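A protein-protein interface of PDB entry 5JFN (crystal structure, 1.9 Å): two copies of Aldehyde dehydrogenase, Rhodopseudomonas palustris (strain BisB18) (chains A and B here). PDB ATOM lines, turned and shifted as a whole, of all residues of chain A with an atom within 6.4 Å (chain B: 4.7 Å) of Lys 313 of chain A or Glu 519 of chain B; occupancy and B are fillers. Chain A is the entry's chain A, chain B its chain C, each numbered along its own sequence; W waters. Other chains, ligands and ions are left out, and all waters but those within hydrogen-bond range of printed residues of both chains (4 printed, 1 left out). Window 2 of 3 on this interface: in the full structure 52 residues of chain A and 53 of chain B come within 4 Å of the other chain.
Among the printed residues, merely in contact across the chains: Lys 313 of chain A with Glu 519 of chain B (3.995 Å), Lys 475 of chain A with Met 517 of chain B (3.6 Å), Asn 476 of chain A with Val 518 of chain B (3.4 Å), Gly 477 of chain A with Val 518 of chain B (3.9 Å), Gly 486 of chain A with Asn 178 of chain B (3.5 Å) and Gly 486 of chain A with Val 518 of chain B (3.7 Å).
Printed residues of chain B within 4 Å of Lys 313 of chain A: Glu 519 (3.995 Å). Of the printed residues of chain A, Glu 519 of chain B touches Lys 313. Printed residues of chain B within 4 Å of Asn 476 of chain A: Val 518 (3.4 Å). Of the printed residues of chain A, Val 518 of chain B touches Lys 475, Asn 476, Gly 477 and Gly 486. Printed residues of chain B within 4 Å of Lys 475 of chain A: Met 517 and Val 518. Ala 520 of chain B touches none of the printed residues of chain A. Pro 478 of chain A touches none of the printed residues of chain B. The nearest printed residue of chain B that does not touch Lys 313 of chain A is Val 518 of chain B (4.7 Å). The nearest printed residue of chain B that does not touch Asn 476 of chain A is Met 517 of chain B (4.5 Å).
N of Val 518 of chain B is in hydrogen-bond range of O of Lys 475 of chain A, 3.0 Å away.
No position is printed for both chains.
Water W2 lies within hydrogen-bond range of O of Val 518 of chain B, ND2 of Asn 476 of chain A and SD of Met 517 of chain B. Water W3 lies within hydrogen-bond range of the backbone carbonyl oxygen (O) of Asn 476 of chain A, the backbone carbonyl oxygen (O) of Val 518 of chain B and the side-chain amino group (NZ) of Lys 313 of chain A. Water W1 bridges the backbone NH (N) of Gly 486 of chain A and the side-chain amide nitrogen (ND2) of Asn 178 of chain B. Water W4 lies within hydrogen-bond range of NZ of Lys 313 of chain A (2.9 Å) and OE2 of Glu 519 of chain B (3.1 Å).
NZ of Lys 313 of chain A is in salt-bridge range of OD2 of Asp 317 of chain A, 2.7 Å away. The backbone NH (N) of Glu 519 of chain B is in hydrogen-bond range of the backbone carbonyl oxygen (O) of Asn 178 of chain B (2.9 Å). The side-chain amino group (NZ) of Lys 313 of chain A lies within hydrogen-bond range of the backbone carbonyl oxygen (O) of Asn 476 of chain A (2.9 Å). The side-chain amide oxygen of Asn 310 of chain A lies within hydrogen-bond range of the backbone NH of Lys 313 of chain A, at 3.1 Å.
Of the 8 printed residues of chain B, 4 touch a printed residue of chain A. Printed residues of chain B that touch a printed residue of chain A: Asn 178, Met 517, Val 518 and Glu 519. Hydrophobic or aromatic side chains of chain B within 4 Å of the printed part of chain A: Met 517 and Val 518. Along chain B the printed residues that touch a printed residue of chain A span positions 178 to 519. Printed residues of chain A that touch a printed residue of chain B: Lys 313, Lys 475, Asn 476, Gly 477 and Gly 486. Among the printed residues, 7 pairs touch across the chains.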
ATOM      1  N   ASN A 310      15.224 -35.860 -23.219  1.00  0.00           N
ATOM      2  CA  ASN A 310      15.429 -35.068 -24.427  1.00  0.00           C
ATOM      3  C   ASN A 310      16.938 -34.962 -24.623  1.00  0.00           C
ATOM      4  O   ASN A 310      17.611 -34.181 -23.946  1.00  0.00           O
ATOM      5  CB  ASN A 310      14.763 -33.701 -24.287  1.00  0.00           C
ATOM      6  CG  ASN A 310      14.891 -32.837 -25.543  1.00  0.00           C
ATOM      7  OD1 ASN A 310      15.811 -33.001 -26.342  1.00  0.00           O
ATOM      8  ND2 ASN A 310      13.965 -31.897 -25.704  1.00  0.00           N
ATOM      9  N   ILE A 311      17.479 -35.765 -25.541  1.00  0.00           N
ATOM     10  CA  ILE A 311      18.930 -35.917 -25.632  1.00  0.00           C
ATOM     11  C   ILE A 311      19.575 -34.657 -26.192  1.00  0.00           C
ATOM     12  O   ILE A 311      20.662 -34.254 -25.756  1.00  0.00           O
ATOM     13  CB  ILE A 311      19.285 -37.155 -26.476  1.00  0.00           C
ATOM     14  CG1 ILE A 311      18.699 -38.419 -25.835  1.00  0.00           C
ATOM     15  CG2 ILE A 311      20.790 -37.279 -26.621  1.00  0.00           C
ATOM     16  CD1 ILE A 311      19.285 -38.738 -24.481  1.00  0.00           C
ATOM     17  N   GLU A 312      18.928 -34.025 -27.174  1.00  0.00           N
ATOM     18  CA  GLU A 312      19.474 -32.796 -27.740  1.00  0.00           C
ATOM     19  C   GLU A 312      19.538 -31.698 -26.685  1.00  0.00           C
ATOM     20  O   GLU A 312      20.549 -30.991 -26.568  1.00  0.00           O
ATOM     21  CB  GLU A 312      18.636 -32.347 -28.938  1.00  0.00           C
ATOM     22  CG  GLU A 312      18.676 -33.310 -30.128  1.00  0.00           C
ATOM     23  CD  GLU A 312      17.667 -34.447 -30.013  1.00  0.00           C
ATOM     24  OE1 GLU A 312      16.939 -34.509 -28.996  1.00  0.00           O
ATOM     25  OE2 GLU A 312      17.598 -35.278 -30.943  1.00  0.00           O
ATOM     26  N   LYS A 313      18.470 -31.551 -25.899  1.00  0.00           N
ATOM     27  CA  LYS A 313      18.486 -30.564 -24.825  1.00  0.00           C
ATOM     28  C   LYS A 313      19.462 -30.969 -23.732  1.00  0.00           C
ATOM     29  O   LYS A 313      20.183 -30.121 -23.195  1.00  0.00           O
ATOM     30  CB  LYS A 313      17.078 -30.378 -24.253  1.00  0.00           C
ATOM     31  CG  LYS A 313      17.020 -29.400 -23.069  1.00  0.00           C
ATOM     32  CD  LYS A 313      15.586 -29.048 -22.683  1.00  0.00           C
ATOM     33  CE  LYS A 313      15.553 -27.828 -21.751  1.00  0.00           C
ATOM     34  NZ  LYS A 313      16.323 -28.043 -20.476  1.00  0.00           N
ATOM     35  N   ALA A 314      19.500 -32.259 -23.389  1.00  0.00           N
ATOM     36  CA  ALA A 314      20.427 -32.718 -22.357  1.00  0.00           C
ATOM     37  C   ALA A 314      21.861 -32.363 -22.718  1.00  0.00           C
ATOM     38  O   ALA A 314      22.625 -31.893 -21.870  1.00  0.00           O
ATOM     39  CB  ALA A 314      20.294 -34.226 -22.149  1.00  0.00           C
ATOM     40  N   ALA A 315      22.245 -32.593 -23.977  1.00  0.00           N
ATOM     41  CA  ALA A 315      23.607 -32.292 -24.396  1.00  0.00           C
ATOM     42  C   ALA A 315      23.922 -30.816 -24.224  1.00  0.00           C
ATOM     43  O   ALA A 315      25.003 -30.453 -23.747  1.00  0.00           O
ATOM     44  CB  ALA A 315      23.815 -32.704 -25.851  1.00  0.00           C
ATOM     45  N   CYS A 316      22.990 -29.951 -24.622  1.00  0.00           N
ATOM     46  CA  CYS A 316      23.205 -28.516 -24.490  1.00  0.00           C
ATOM     47  C   CYS A 316      23.296 -28.113 -23.023  1.00  0.00           C
ATOM     48  O   CYS A 316      24.226 -27.402 -22.620  1.00  0.00           O
ATOM     49  CB  CYS A 316      22.077 -27.762 -25.195  1.00  0.00           C
ATOM     50  SG  CYS A 316      22.144 -25.976 -24.995  1.00  0.00           S
ATOM     51  N   ASP A 317      22.345 -28.580 -22.204  1.00  0.00           N
ATOM     52  CA  ASP A 317      22.359 -28.276 -20.773  1.00  0.00           C
ATOM     53  C   ASP A 317      23.649 -28.747 -20.118  1.00  0.00           C
ATOM     54  O   ASP A 317      24.205 -28.060 -19.251  1.00  0.00           O
ATOM     55  CB  ASP A 317      21.161 -28.933 -20.077  1.00  0.00           C
ATOM     56  CG  ASP A 317      19.839 -28.341 -20.497  1.00  0.00           C
ATOM     57  OD1 ASP A 317      19.836 -27.237 -21.080  1.00  0.00           O
ATOM     58  OD2 ASP A 317      18.795 -28.973 -20.225  1.00  0.00           O
ATOM     59  N   ILE A 318      24.127 -29.931 -20.500  1.00  0.00           N
ATOM     60  CA  ILE A 318      25.293 -30.503 -19.841  1.00  0.00           C
ATOM     61  C   ILE A 318      26.549 -29.719 -20.197  1.00  0.00           C
ATOM     62  O   ILE A 318      27.388 -29.444 -19.334  1.00  0.00           O
ATOM     63  CB  ILE A 318      25.429 -31.992 -20.201  1.00  0.00           C
ATOM     64  CG1 ILE A 318      24.342 -32.804 -19.483  1.00  0.00           C
ATOM     65  CG2 ILE A 318      26.778 -32.505 -19.815  1.00  0.00           C
ATOM     66  CD1 ILE A 318      24.258 -34.248 -19.959  1.00  0.00           C
ATOM     67  N   ASN A 349      25.624 -35.363 -29.708  1.00  0.00           N
ATOM     68  CA  ASN A 349      25.049 -34.044 -29.467  1.00  0.00           C
ATOM     69  C   ASN A 349      25.922 -33.190 -28.559  1.00  0.00           C
ATOM     70  O   ASN A 349      25.934 -31.961 -28.699  1.00  0.00           O
ATOM     71  CB  ASN A 349      23.644 -34.192 -28.889  1.00  0.00           C
ATOM     72  CG  ASN A 349      22.627 -34.541 -29.945  1.00  0.00           C
ATOM     73  OD1 ASN A 349      22.125 -33.661 -30.645  1.00  0.00           O
ATOM     74  ND2 ASN A 349      22.316 -35.831 -30.073  1.00  0.00           N
ATOM     75  N   HIS A 454      18.739 -36.092 -16.453  1.00  0.00           N
ATOM     76  CA  HIS A 454      17.910 -35.854 -17.629  1.00  0.00           C
ATOM     77  C   HIS A 454      17.107 -37.118 -17.883  1.00  0.00           C
ATOM     78  O   HIS A 454      17.670 -38.173 -18.183  1.00  0.00           O
ATOM     79  CB  HIS A 454      18.755 -35.459 -18.836  1.00  0.00           C
ATOM     80  CG  HIS A 454      19.503 -34.178 -18.627  1.00  0.00           C
ATOM     81  ND1 HIS A 454      19.003 -32.953 -19.013  1.00  0.00           N
ATOM     82  CD2 HIS A 454      20.698 -33.930 -18.039  1.00  0.00           C
ATOM     83  CE1 HIS A 454      19.868 -32.004 -18.689  1.00  0.00           C
ATOM     84  NE2 HIS A 454      20.907 -32.571 -18.099  1.00  0.00           N
ATOM     85  N   LYS A 475      16.589 -31.454 -12.410  1.00  0.00           N
ATOM     86  CA  LYS A 475      15.990 -32.360 -13.374  1.00  0.00           C
ATOM     87  C   LYS A 475      15.798 -31.625 -14.693  1.00  0.00           C
ATOM     88  O   LYS A 475      15.112 -30.599 -14.740  1.00  0.00           O
ATOM     89  CB  LYS A 475      14.660 -32.901 -12.845  1.00  0.00           C
ATOM     90  CG  LYS A 475      14.841 -33.823 -11.654  1.00  0.00           C
ATOM     91  CD  LYS A 475      13.562 -33.992 -10.857  1.00  0.00           C
ATOM     92  CE  LYS A 475      13.179 -32.673 -10.209  1.00  0.00           C
ATOM     93  NZ  LYS A 475      12.235 -32.834  -9.071  1.00  0.00           N
ATOM     94  N   ASN A 476      16.414 -32.150 -15.755  1.00  0.00           N
ATOM     95  CA  ASN A 476      16.172 -31.675 -17.117  1.00  0.00           C
ATOM     96  C   ASN A 476      16.580 -30.214 -17.293  1.00  0.00           C
ATOM     97  O   ASN A 476      15.890 -29.425 -17.946  1.00  0.00           O
ATOM     98  CB  ASN A 476      14.714 -31.899 -17.506  1.00  0.00           C
ATOM     99  CG  ASN A 476      14.338 -33.354 -17.441  1.00  0.00           C
ATOM    100  OD1 ASN A 476      15.126 -34.215 -17.834  1.00  0.00           O
ATOM    101  ND2 ASN A 476      13.157 -33.648 -16.910  1.00  0.00           N
ATOM    102  N   GLY A 477      17.711 -29.853 -16.712  1.00  0.00           N
ATOM    103  CA  GLY A 477      18.264 -28.539 -16.917  1.00  0.00           C
ATOM    104  C   GLY A 477      19.732 -28.510 -16.570  1.00  0.00           C
ATOM    105  O   GLY A 477      20.277 -29.464 -16.003  1.00  0.00           O
ATOM    106  N   PRO A 478      20.411 -27.417 -16.912  1.00  0.00           N
ATOM    107  CA  PRO A 478      21.795 -27.249 -16.455  1.00  0.00           C
ATOM    108  C   PRO A 478      21.842 -27.197 -14.938  1.00  0.00           C
ATOM    109  O   PRO A 478      20.883 -26.787 -14.276  1.00  0.00           O
ATOM    110  CB  PRO A 478      22.224 -25.915 -17.081  1.00  0.00           C
ATOM    111  CG  PRO A 478      20.936 -25.191 -17.349  1.00  0.00           C
ATOM    112  CD  PRO A 478      19.915 -26.244 -17.654  1.00  0.00           C
ATOM    113  N   GLY A 486      17.474 -20.158 -14.370  1.00  0.00           N
ATOM    114  CA  GLY A 486      16.691 -21.116 -15.132  1.00  0.00           C
ATOM    115  C   GLY A 486      15.965 -22.148 -14.296  1.00  0.00           C
ATOM    116  O   GLY A 486      15.456 -23.132 -14.853  1.00  0.00           O
ATOM    117  N   ASP B 177       7.601 -20.061 -14.568  1.00  0.00           N
ATOM    118  CA  ASP B 177       8.051 -20.327 -15.928  1.00  0.00           C
ATOM    119  C   ASP B 177       9.202 -21.322 -15.970  1.00  0.00           C
ATOM    120  O   ASP B 177       9.379 -22.017 -16.975  1.00  0.00           O
ATOM    121  CB  ASP B 177       8.466 -19.021 -16.610  1.00  0.00           C
ATOM    122  CG  ASP B 177       7.315 -18.045 -16.749  1.00  0.00           C
ATOM    123  OD1 ASP B 177       6.147 -18.494 -16.761  1.00  0.00           O
ATOM    124  OD2 ASP B 177       7.582 -16.828 -16.864  1.00  0.00           O
ATOM    125  N   ASN B 178      10.008 -21.390 -14.915  1.00  0.00           N
ATOM    126  CA  ASN B 178      11.148 -22.296 -14.880  1.00  0.00           C
ATOM    127  C   ASN B 178      10.795 -23.655 -14.303  1.00  0.00           C
ATOM    128  O   ASN B 178      11.696 -24.466 -14.067  1.00  0.00           O
ATOM    129  CB  ASN B 178      12.294 -21.675 -14.082  1.00  0.00           C
ATOM    130  CG  ASN B 178      12.905 -20.477 -14.782  1.00  0.00           C
ATOM    131  OD1 ASN B 178      13.227 -20.537 -15.967  1.00  0.00           O
ATOM    132  ND2 ASN B 178      13.053 -19.380 -14.055  1.00  0.00           N
ATOM    133  N   GLY B 179       9.513 -23.920 -14.073  1.00  0.00           N
ATOM    134  CA  GLY B 179       9.076 -25.230 -13.632  1.00  0.00           C
ATOM    135  C   GLY B 179       8.658 -25.235 -12.179  1.00  0.00           C
ATOM    136  O   GLY B 179       7.916 -24.355 -11.732  1.00  0.00           O
ATOM    137  N   MET B 517      12.616 -29.107 -10.720  1.00  0.00           N
ATOM    138  CA  MET B 517      12.063 -29.702 -11.934  1.00  0.00           C
ATOM    139  C   MET B 517      12.026 -28.612 -12.994  1.00  0.00           C
ATOM    140  O   MET B 517      11.112 -27.785 -13.017  1.00  0.00           O
ATOM    141  CB  MET B 517      10.677 -30.276 -11.670  1.00  0.00           C
ATOM    142  CG  MET B 517      10.034 -30.889 -12.898  1.00  0.00           C
ATOM    143  SD  MET B 517      10.715 -32.515 -13.270  1.00  0.00           S
ATOM    144  CE  MET B 517       9.942 -33.501 -11.982  1.00  0.00           C
ATOM    145  N   VAL B 518      13.030 -28.600 -13.868  1.00  0.00           N
ATOM    146  CA  VAL B 518      13.189 -27.496 -14.808  1.00  0.00           C
ATOM    147  C   VAL B 518      12.117 -27.594 -15.887  1.00  0.00           C
ATOM    148  O   VAL B 518      12.031 -28.596 -16.608  1.00  0.00           O
ATOM    149  CB  VAL B 518      14.600 -27.491 -15.416  1.00  0.00           C
ATOM    150  CG1 VAL B 518      14.733 -26.367 -16.430  1.00  0.00           C
ATOM    151  CG2 VAL B 518      15.660 -27.357 -14.313  1.00  0.00           C
ATOM    152  N   GLU B 519      11.280 -26.556 -15.973  1.00  0.00           N
ATOM    153  CA  GLU B 519      10.295 -26.374 -17.046  1.00  0.00           C
ATOM    154  C   GLU B 519       9.279 -27.510 -17.109  1.00  0.00           C
ATOM    155  O   GLU B 519       8.830 -27.896 -18.189  1.00  0.00           O
ATOM    156  CB  GLU B 519      10.985 -26.185 -18.399  1.00  0.00           C
ATOM    157  CG  GLU B 519      11.682 -24.837 -18.498  1.00  0.00           C
ATOM    158  CD  GLU B 519      12.651 -24.748 -19.654  1.00  0.00           C
ATOM    159  OE1 GLU B 519      12.499 -25.510 -20.627  1.00  0.00           O
ATOM    160  OE2 GLU B 519      13.576 -23.918 -19.576  1.00  0.00           O
ATOM    161  N   ALA B 520       8.907 -28.045 -15.950  1.00  0.00           N
ATOM    162  CA  ALA B 520       7.804 -28.985 -15.848  1.00  0.00           C
ATOM    163  C   ALA B 520       7.208 -28.855 -14.456  1.00  0.00           C
ATOM    164  O   ALA B 520       7.790 -28.228 -13.563  1.00  0.00           O
ATOM    165  CB  ALA B 520       8.249 -30.427 -16.135  1.00  0.00           C
ATOM    166  N   ASN B 522       4.831 -27.100 -13.550  1.00  0.00           N
ATOM    167  CA  ASN B 522       4.308 -25.758 -13.323  1.00  0.00           C
ATOM    168  C   ASN B 522       2.897 -25.744 -13.907  1.00  0.00           C
ATOM    169  O   ASN B 522       2.679 -25.361 -15.056  1.00  0.00           O
ATOM    170  CB  ASN B 522       5.216 -24.701 -13.944  1.00  0.00           C
ATOM    171  CG  ASN B 522       5.524 -24.960 -15.415  1.00  0.00           C
ATOM    172  OD1 ASN B 522       5.708 -26.105 -15.848  1.00  0.00           O
ATOM    173  ND2 ASN B 522       5.569 -23.884 -16.194  1.00  0.00           N
HETATM  174  O   HOH W   1      15.977 -17.741 -14.168  1.00  0.00           O
HETATM  175  O   HOH W   2      11.529 -31.309 -16.351  1.00  0.00           O
HETATM  176  O   HOH W   3      13.368 -29.182 -19.138  1.00  0.00           O
HETATM  177  O   HOH W   4      16.331 -25.414 -19.285  1.00  0.00           O
